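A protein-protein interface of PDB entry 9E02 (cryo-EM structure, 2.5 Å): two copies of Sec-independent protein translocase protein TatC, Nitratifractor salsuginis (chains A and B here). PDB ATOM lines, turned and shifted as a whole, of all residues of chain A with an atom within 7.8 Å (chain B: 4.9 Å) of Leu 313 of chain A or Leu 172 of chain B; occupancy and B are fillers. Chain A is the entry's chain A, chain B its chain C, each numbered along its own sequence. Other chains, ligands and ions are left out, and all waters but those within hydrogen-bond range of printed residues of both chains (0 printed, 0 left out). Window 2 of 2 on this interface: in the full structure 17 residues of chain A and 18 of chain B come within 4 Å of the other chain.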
ATOM      1  N   LEU A 237      -8.581   6.203  22.326  1.00  0.00           N
ATOM      2  CA  LEU A 237      -8.294   7.560  22.768  1.00  0.00           C
ATOM      3  C   LEU A 237      -9.416   8.129  23.632  1.00  0.00           C
ATOM      4  O   LEU A 237      -9.146   8.846  24.602  1.00  0.00           O
ATOM      5  CB  LEU A 237      -8.024   8.446  21.560  1.00  0.00           C
ATOM      6  CG  LEU A 237      -6.773   8.169  20.725  1.00  0.00           C
ATOM      7  CD1 LEU A 237      -6.756   9.026  19.478  1.00  0.00           C
ATOM      8  CD2 LEU A 237      -5.520   8.403  21.538  1.00  0.00           C
ATOM      9  N   PHE A 240      -9.126   6.447  26.987  1.00  0.00           N
ATOM     10  CA  PHE A 240      -7.949   6.831  27.756  1.00  0.00           C
ATOM     11  C   PHE A 240      -8.287   7.871  28.816  1.00  0.00           C
ATOM     12  O   PHE A 240      -7.829   7.772  29.960  1.00  0.00           O
ATOM     13  CB  PHE A 240      -6.855   7.349  26.823  1.00  0.00           C
ATOM     14  CG  PHE A 240      -5.505   7.424  27.469  1.00  0.00           C
ATOM     15  CD1 PHE A 240      -4.674   6.321  27.494  1.00  0.00           C
ATOM     16  CD2 PHE A 240      -5.074   8.593  28.065  1.00  0.00           C
ATOM     17  CE1 PHE A 240      -3.437   6.386  28.095  1.00  0.00           C
ATOM     18  CE2 PHE A 240      -3.838   8.661  28.664  1.00  0.00           C
ATOM     19  CZ  PHE A 240      -3.019   7.558  28.678  1.00  0.00           C
ATOM     20  N   THR A 308       3.613  20.364  12.094  1.00  0.00           N
ATOM     21  CA  THR A 308       3.051  20.279  13.430  1.00  0.00           C
ATOM     22  C   THR A 308       3.062  21.650  14.085  1.00  0.00           C
ATOM     23  O   THR A 308       3.782  22.551  13.644  1.00  0.00           O
ATOM     24  CB  THR A 308       3.838  19.285  14.300  1.00  0.00           C
ATOM     25  OG1 THR A 308       5.235  19.590  14.235  1.00  0.00           O
ATOM     26  CG2 THR A 308       3.617  17.866  13.827  1.00  0.00           C
ATOM     27  N   PRO A 309       2.258  21.846  15.127  1.00  0.00           N
ATOM     28  CA  PRO A 309       2.345  23.075  15.921  1.00  0.00           C
ATOM     29  C   PRO A 309       3.735  23.250  16.506  1.00  0.00           C
ATOM     30  O   PRO A 309       4.530  22.299  16.538  1.00  0.00           O
ATOM     31  CB  PRO A 309       1.298  22.851  17.022  1.00  0.00           C
ATOM     32  CG  PRO A 309       0.312  21.940  16.403  1.00  0.00           C
ATOM     33  CD  PRO A 309       1.091  21.030  15.508  1.00  0.00           C
ATOM     34  N   PRO A 310       4.070  24.453  16.994  1.00  0.00           N
ATOM     35  CA  PRO A 310       5.450  24.719  17.431  1.00  0.00           C
ATOM     36  C   PRO A 310       5.918  23.924  18.645  1.00  0.00           C
ATOM     37  O   PRO A 310       7.042  24.126  19.113  1.00  0.00           O
ATOM     38  CB  PRO A 310       5.430  26.221  17.738  1.00  0.00           C
ATOM     39  CG  PRO A 310       4.280  26.755  16.965  1.00  0.00           C
ATOM     40  CD  PRO A 310       3.256  25.678  16.979  1.00  0.00           C
ATOM     41  N   ASP A 311       5.085  23.030  19.166  1.00  0.00           N
ATOM     42  CA  ASP A 311       5.493  22.199  20.290  1.00  0.00           C
ATOM     43  C   ASP A 311       6.487  21.132  19.842  1.00  0.00           C
ATOM     44  O   ASP A 311       6.400  20.604  18.730  1.00  0.00           O
ATOM     45  CB  ASP A 311       4.272  21.543  20.931  1.00  0.00           C
ATOM     46  CG  ASP A 311       3.076  22.471  20.989  1.00  0.00           C
ATOM     47  OD1 ASP A 311       3.276  23.697  21.121  1.00  0.00           O
ATOM     48  OD2 ASP A 311       1.932  21.975  20.902  1.00  0.00           O
ATOM     49  N   VAL A 312       7.438  20.814  20.723  1.00  0.00           N
ATOM     50  CA  VAL A 312       8.440  19.797  20.414  1.00  0.00           C
ATOM     51  C   VAL A 312       7.827  18.402  20.460  1.00  0.00           C
ATOM     52  O   VAL A 312       8.191  17.523  19.668  1.00  0.00           O
ATOM     53  CB  VAL A 312       9.639  19.929  21.370  1.00  0.00           C
ATOM     54  CG1 VAL A 312      10.428  18.635  21.440  1.00  0.00           C
ATOM     55  CG2 VAL A 312      10.534  21.058  20.925  1.00  0.00           C
ATOM     56  N   LEU A 313       6.894  18.172  21.387  1.00  0.00           N
ATOM     57  CA  LEU A 313       6.323  16.838  21.545  1.00  0.00           C
ATOM     58  C   LEU A 313       5.565  16.403  20.296  1.00  0.00           C
ATOM     59  O   LEU A 313       5.667  15.245  19.875  1.00  0.00           O
ATOM     60  CB  LEU A 313       5.417  16.795  22.772  1.00  0.00           C
ATOM     61  CG  LEU A 313       4.931  15.398  23.157  1.00  0.00           C
ATOM     62  CD1 LEU A 313       6.082  14.531  23.623  1.00  0.00           C
ATOM     63  CD2 LEU A 313       3.873  15.492  24.227  1.00  0.00           C
ATOM     64  N   THR A 314       4.805  17.315  19.688  1.00  0.00           N
ATOM     65  CA  THR A 314       4.168  17.008  18.413  1.00  0.00           C
ATOM     66  C   THR A 314       5.207  16.704  17.343  1.00  0.00           C
ATOM     67  O   THR A 314       5.004  15.821  16.500  1.00  0.00           O
ATOM     68  CB  THR A 314       3.274  18.167  17.973  1.00  0.00           C
ATOM     69  OG1 THR A 314       3.842  19.407  18.412  1.00  0.00           O
ATOM     70  CG2 THR A 314       1.879  18.019  18.543  1.00  0.00           C
ATOM     71  N   GLN A 315       6.330  17.419  17.367  1.00  0.00           N
ATOM     72  CA  GLN A 315       7.389  17.177  16.396  1.00  0.00           C
ATOM     73  C   GLN A 315       7.951  15.767  16.528  1.00  0.00           C
ATOM     74  O   GLN A 315       8.162  15.081  15.523  1.00  0.00           O
ATOM     75  CB  GLN A 315       8.493  18.218  16.571  1.00  0.00           C
ATOM     76  CG  GLN A 315       9.530  18.220  15.478  1.00  0.00           C
ATOM     77  CD  GLN A 315      10.779  18.956  15.874  1.00  0.00           C
ATOM     78  OE1 GLN A 315      10.946  19.335  17.028  1.00  0.00           O
ATOM     79  NE2 GLN A 315      11.662  19.179  14.914  1.00  0.00           N
ATOM     80  N   LEU A 316       8.187  15.310  17.758  1.00  0.00           N
ATOM     81  CA  LEU A 316       8.684  13.950  17.950  1.00  0.00           C
ATOM     82  C   LEU A 316       7.623  12.916  17.586  1.00  0.00           C
ATOM     83  O   LEU A 316       7.934  11.876  16.987  1.00  0.00           O
ATOM     84  CB  LEU A 316       9.150  13.758  19.392  1.00  0.00           C
ATOM     85  CG  LEU A 316      10.043  14.844  19.993  1.00  0.00           C
ATOM     86  CD1 LEU A 316       9.998  14.785  21.508  1.00  0.00           C
ATOM     87  CD2 LEU A 316      11.467  14.713  19.495  1.00  0.00           C
ATOM     88  N   LEU A 317       6.363  13.191  17.937  1.00  0.00           N
ATOM     89  CA  LEU A 317       5.277  12.271  17.624  1.00  0.00           C
ATOM     90  C   LEU A 317       5.064  12.137  16.125  1.00  0.00           C
ATOM     91  O   LEU A 317       4.562  11.109  15.662  1.00  0.00           O
ATOM     92  CB  LEU A 317       3.986  12.741  18.292  1.00  0.00           C
ATOM     93  CG  LEU A 317       3.820  12.496  19.791  1.00  0.00           C
ATOM     94  CD1 LEU A 317       2.408  12.842  20.220  1.00  0.00           C
ATOM     95  CD2 LEU A 317       4.157  11.063  20.151  1.00  0.00           C
ATOM     96  N   MET A 318       5.407  13.168  15.357  1.00  0.00           N
ATOM     97  CA  MET A 318       5.333  13.084  13.904  1.00  0.00           C
ATOM     98  C   MET A 318       6.606  12.521  13.288  1.00  0.00           C
ATOM     99  O   MET A 318       6.547  11.895  12.223  1.00  0.00           O
ATOM    100  CB  MET A 318       5.032  14.464  13.314  1.00  0.00           C
ATOM    101  CG  MET A 318       4.924  14.499  11.798  1.00  0.00           C
ATOM    102  SD  MET A 318       3.323  13.938  11.190  1.00  0.00           S
ATOM    103  CE  MET A 318       2.361  15.441  11.319  1.00  0.00           C
ATOM    104  N   ALA A 319       7.754  12.718  13.934  1.00  0.00           N
ATOM    105  CA  ALA A 319       9.001  12.182  13.406  1.00  0.00           C
ATOM    106  C   ALA A 319       9.063  10.668  13.550  1.00  0.00           C
ATOM    107  O   ALA A 319       9.616   9.983  12.682  1.00  0.00           O
ATOM    108  CB  ALA A 319      10.190  12.835  14.105  1.00  0.00           C
ATOM    109  N   PHE B  27      10.917  10.406  30.753  1.00  0.00           N
ATOM    110  CA  PHE B  27       9.611  10.330  30.109  1.00  0.00           C
ATOM    111  C   PHE B  27       8.960   8.979  30.350  1.00  0.00           C
ATOM    112  O   PHE B  27       7.747   8.899  30.559  1.00  0.00           O
ATOM    113  CB  PHE B  27       9.740  10.607  28.609  1.00  0.00           C
ATOM    114  CG  PHE B  27       8.540  10.183  27.810  1.00  0.00           C
ATOM    115  CD1 PHE B  27       7.510  11.072  27.570  1.00  0.00           C
ATOM    116  CD2 PHE B  27       8.447   8.903  27.282  1.00  0.00           C
ATOM    117  CE1 PHE B  27       6.408  10.693  26.845  1.00  0.00           C
ATOM    118  CE2 PHE B  27       7.343   8.519  26.557  1.00  0.00           C
ATOM    119  CZ  PHE B  27       6.324   9.416  26.336  1.00  0.00           C
ATOM    120  N   PHE B  31       5.504   8.607  32.290  1.00  0.00           N
ATOM    121  CA  PHE B  31       4.312   8.023  31.686  1.00  0.00           C
ATOM    122  C   PHE B  31       3.829   6.818  32.474  1.00  0.00           C
ATOM    123  O   PHE B  31       2.635   6.504  32.453  1.00  0.00           O
ATOM    124  CB  PHE B  31       4.560   7.635  30.232  1.00  0.00           C
ATOM    125  CG  PHE B  31       3.298   7.436  29.451  1.00  0.00           C
ATOM    126  CD1 PHE B  31       2.653   8.509  28.870  1.00  0.00           C
ATOM    127  CD2 PHE B  31       2.738   6.179  29.323  1.00  0.00           C
ATOM    128  CE1 PHE B  31       1.488   8.332  28.165  1.00  0.00           C
ATOM    129  CE2 PHE B  31       1.571   5.998  28.620  1.00  0.00           C
ATOM    130  CZ  PHE B  31       0.946   7.075  28.040  1.00  0.00           C
ATOM    131  N   PHE B 168      -4.904  11.916  25.435  1.00  0.00           N
ATOM    132  CA  PHE B 168      -3.663  11.157  25.272  1.00  0.00           C
ATOM    133  C   PHE B 168      -2.449  12.080  25.228  1.00  0.00           C
ATOM    134  O   PHE B 168      -1.420  11.816  25.861  1.00  0.00           O
ATOM    135  CB  PHE B 168      -3.718  10.283  24.022  1.00  0.00           C
ATOM    136  CG  PHE B 168      -2.636   9.244  23.978  1.00  0.00           C
ATOM    137  CD1 PHE B 168      -2.440   8.387  25.044  1.00  0.00           C
ATOM    138  CD2 PHE B 168      -1.791   9.148  22.888  1.00  0.00           C
ATOM    139  CE1 PHE B 168      -1.440   7.442  25.013  1.00  0.00           C
ATOM    140  CE2 PHE B 168      -0.791   8.205  22.856  1.00  0.00           C
ATOM    141  CZ  PHE B 168      -0.616   7.351  23.920  1.00  0.00           C
ATOM    142  N   PHE B 169      -2.558  13.182  24.489  1.00  0.00           N
ATOM    143  CA  PHE B 169      -1.473  14.136  24.360  1.00  0.00           C
ATOM    144  C   PHE B 169      -1.241  14.883  25.661  1.00  0.00           C
ATOM    145  O   PHE B 169      -0.125  15.322  25.929  1.00  0.00           O
ATOM    146  CB  PHE B 169      -1.795  15.115  23.233  1.00  0.00           C
ATOM    147  CG  PHE B 169      -0.627  15.936  22.789  1.00  0.00           C
ATOM    148  CD1 PHE B 169      -0.598  17.299  23.010  1.00  0.00           C
ATOM    149  CD2 PHE B 169       0.434  15.346  22.128  1.00  0.00           C
ATOM    150  CE1 PHE B 169       0.472  18.054  22.594  1.00  0.00           C
ATOM    151  CE2 PHE B 169       1.506  16.098  21.709  1.00  0.00           C
ATOM    152  CZ  PHE B 169       1.528  17.453  21.946  1.00  0.00           C
ATOM    153  N   VAL B 170      -2.280  15.054  26.478  1.00  0.00           N
ATOM    154  CA  VAL B 170      -2.083  15.670  27.786  1.00  0.00           C
ATOM    155  C   VAL B 170      -1.246  14.757  28.668  1.00  0.00           C
ATOM    156  O   VAL B 170      -0.317  15.204  29.353  1.00  0.00           O
ATOM    157  CB  VAL B 170      -3.441  16.010  28.429  1.00  0.00           C
ATOM    158  CG1 VAL B 170      -3.337  16.010  29.933  1.00  0.00           C
ATOM    159  CG2 VAL B 170      -3.920  17.360  27.943  1.00  0.00           C
ATOM    160  N   ALA B 171      -1.544  13.456  28.640  1.00  0.00           N
ATOM    161  CA  ALA B 171      -0.700  12.503  29.354  1.00  0.00           C
ATOM    162  C   ALA B 171       0.734  12.544  28.837  1.00  0.00           C
ATOM    163  O   ALA B 171       1.690  12.551  29.624  1.00  0.00           O
ATOM    164  CB  ALA B 171      -1.277  11.095  29.233  1.00  0.00           C
ATOM    165  N   LEU B 172       0.902  12.596  27.514  1.00  0.00           N
ATOM    166  CA  LEU B 172       2.241  12.625  26.931  1.00  0.00           C
ATOM    167  C   LEU B 172       2.984  13.911  27.291  1.00  0.00           C
ATOM    168  O   LEU B 172       4.184  13.888  27.571  1.00  0.00           O
ATOM    169  CB  LEU B 172       2.157  12.460  25.414  1.00  0.00           C
ATOM    170  CG  LEU B 172       1.813  11.071  24.878  1.00  0.00           C
ATOM    171  CD1 LEU B 172       1.403  11.156  23.418  1.00  0.00           C
ATOM    172  CD2 LEU B 172       2.970  10.111  25.062  1.00  0.00           C
ATOM    173  N   LYS B 173       2.282  15.046  27.276  1.00  0.00           N
ATOM    174  CA  LYS B 173       2.881  16.335  27.611  1.00  0.00           C
ATOM    175  C   LYS B 173       3.336  16.361  29.060  1.00  0.00           C
ATOM    176  O   LYS B 173       4.438  16.830  29.373  1.00  0.00           O
ATOM    177  CB  LYS B 173       1.857  17.445  27.373  1.00  0.00           C
ATOM    178  CG  LYS B 173       1.702  17.891  25.931  1.00  0.00           C
ATOM    179  CD  LYS B 173       0.914  19.191  25.818  1.00  0.00           C
ATOM    180  CE  LYS B 173       1.432  20.271  26.732  1.00  0.00           C
ATOM    181  NZ  LYS B 173       2.908  20.312  26.653  1.00  0.00           N
ATOM    182  N   VAL B 174       2.483  15.870  29.958  1.00  0.00           N
ATOM    183  CA  VAL B 174       2.827  15.822  31.371  1.00  0.00           C
ATOM    184  C   VAL B 174       4.030  14.918  31.589  1.00  0.00           C
ATOM    185  O   VAL B 174       4.958  15.263  32.332  1.00  0.00           O
ATOM    186  CB  VAL B 174       1.600  15.365  32.182  1.00  0.00           C
ATOM    187  CG1 VAL B 174       2.019  14.655  33.444  1.00  0.00           C
ATOM    188  CG2 VAL B 174       0.712  16.553  32.493  1.00  0.00           C
ATOM    189  N   SER B 175       4.044  13.758  30.928  1.00  0.00           N
ATOM    190  CA  SER B 175       5.180  12.853  31.052  1.00  0.00           C
ATOM    191  C   SER B 175       6.455  13.478  30.502  1.00  0.00           C
ATOM    192  O   SER B 175       7.532  13.307  31.078  1.00  0.00           O
ATOM    193  CB  SER B 175       4.878  11.535  30.347  1.00  0.00           C
ATOM    194  OG  SER B 175       3.534  11.149  30.556  1.00  0.00           O
ATOM    195  N   PHE B 176       6.355  14.208  29.394  1.00  0.00           N
ATOM    196  CA  PHE B 176       7.526  14.850  28.806  1.00  0.00           C
ATOM    197  C   PHE B 176       8.100  15.921  29.725  1.00  0.00           C
ATOM    198  O   PHE B 176       9.318  15.993  29.931  1.00  0.00           O
ATOM    199  CB  PHE B 176       7.155  15.444  27.449  1.00  0.00           C
ATOM    200  CG  PHE B 176       8.334  15.801  26.606  1.00  0.00           C
ATOM    201  CD1 PHE B 176       8.416  17.042  26.007  1.00  0.00           C
ATOM    202  CD2 PHE B 176       9.364  14.903  26.415  1.00  0.00           C
ATOM    203  CE1 PHE B 176       9.500  17.380  25.235  1.00  0.00           C
ATOM    204  CE2 PHE B 176      10.452  15.237  25.644  1.00  0.00           C
ATOM    205  CZ  PHE B 176      10.518  16.476  25.052  1.00  0.00           C
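The backbone carbonyl oxygen (O) of Asp 311 of chain A sits at hydrogen-bond distance from the side-chain hydroxyl (OG1) of Thr 314 of chain A, 2.8 Å away.
The side-chain hydroxyl (OG) of Ser 175 of chain B is in hydrogen-bond range of the backbone carbonyl oxygen (O) of Ala 171 of chain B (2.5 Å).
Of the printed residues of chain B, Phe 240 of chain A touches Phe 168 (3.8 Å) and Ala 171 (3.6 Å).
Val 312 of chain A touches none of the printed residues of chain B.
Leu 313 of chain A touches just these residues of chain B: Phe 169, Leu 172, Lys 173 and Phe 176.
Of the printed residues of chain A, Phe 168 of chain B touches Leu 237 and Phe 240.
Printed residues of chain A within 4 Å of Phe 169 of chain B: Leu 313 (3.5 Å), Thr 314 (3.5 Å) and Leu 317 (3.7 Å).
Val 170 of chain B touches none of the printed residues of chain A.
Ala 171 of chain B touches just one residue of chain A: Phe 240.
Printed residues of chain A within 4 Å of Lys 173 of chain B: Leu 313 (3.5 Å).
Printed residues of chain A within 4 Å of Phe 176 of chain B: Leu 313 and Leu 316.
The nearest printed residue of chain B that does not touch Leu 313 of chain A is Phe 27 of chain B (5.0 Å).
The nearest residue of chain A that does not touch Leu 172 of chain B is Phe 240 of chain A (6.3 Å).
The nearest printed residue of chain A that does not touch Phe 176 of chain B is Val 312 of chain A (4.1 Å).
Of the 11 printed residues of chain B, 6 touch a printed residue of chain A.
Hydrophobic or aromatic side chains of chain B that line the printed part of chain A: Phe 168, Phe 169, Ala 171, Leu 172 and Phe 176.
Of the 14 printed residues of chain A, 6 touch a printed residue of chain B.
Printed residues of chain A that touch a printed residue of chain B: Leu 237, Phe 240, Leu 313, Thr 314, Leu 316 and Leu 317.
No position is printed for both chains.
Among the printed residues, merely in contact across the chains: Leu 237 of chain A with Phe 168 of chain B (3.6 Å), Phe 240 of chain A with Phe 168 of chain B (3.8 Å), Phe 240 of chain A with Ala 171 of chain B (3.6 Å), Leu 313 of chain A with Phe 169 of chain B (3.5 Å), Leu 313 of chain A with Leu 172 of chain B (3.6 Å), Leu 313 of chain A with Lys 173 of chain B (3.5 Å), Leu 313 of chain A with Phe 176 of chain B (3.9 Å), Thr 314 of chain A with Phe 169 of chain B (3.5 Å), Leu 316 of chain A with Phe 176 of chain B (3.96 Å), Leu 317 of chain A with Phe 169 of chain B (3.7 Å) and Leu 317 of chain A with Leu 172 of chain B (3.8 Å).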
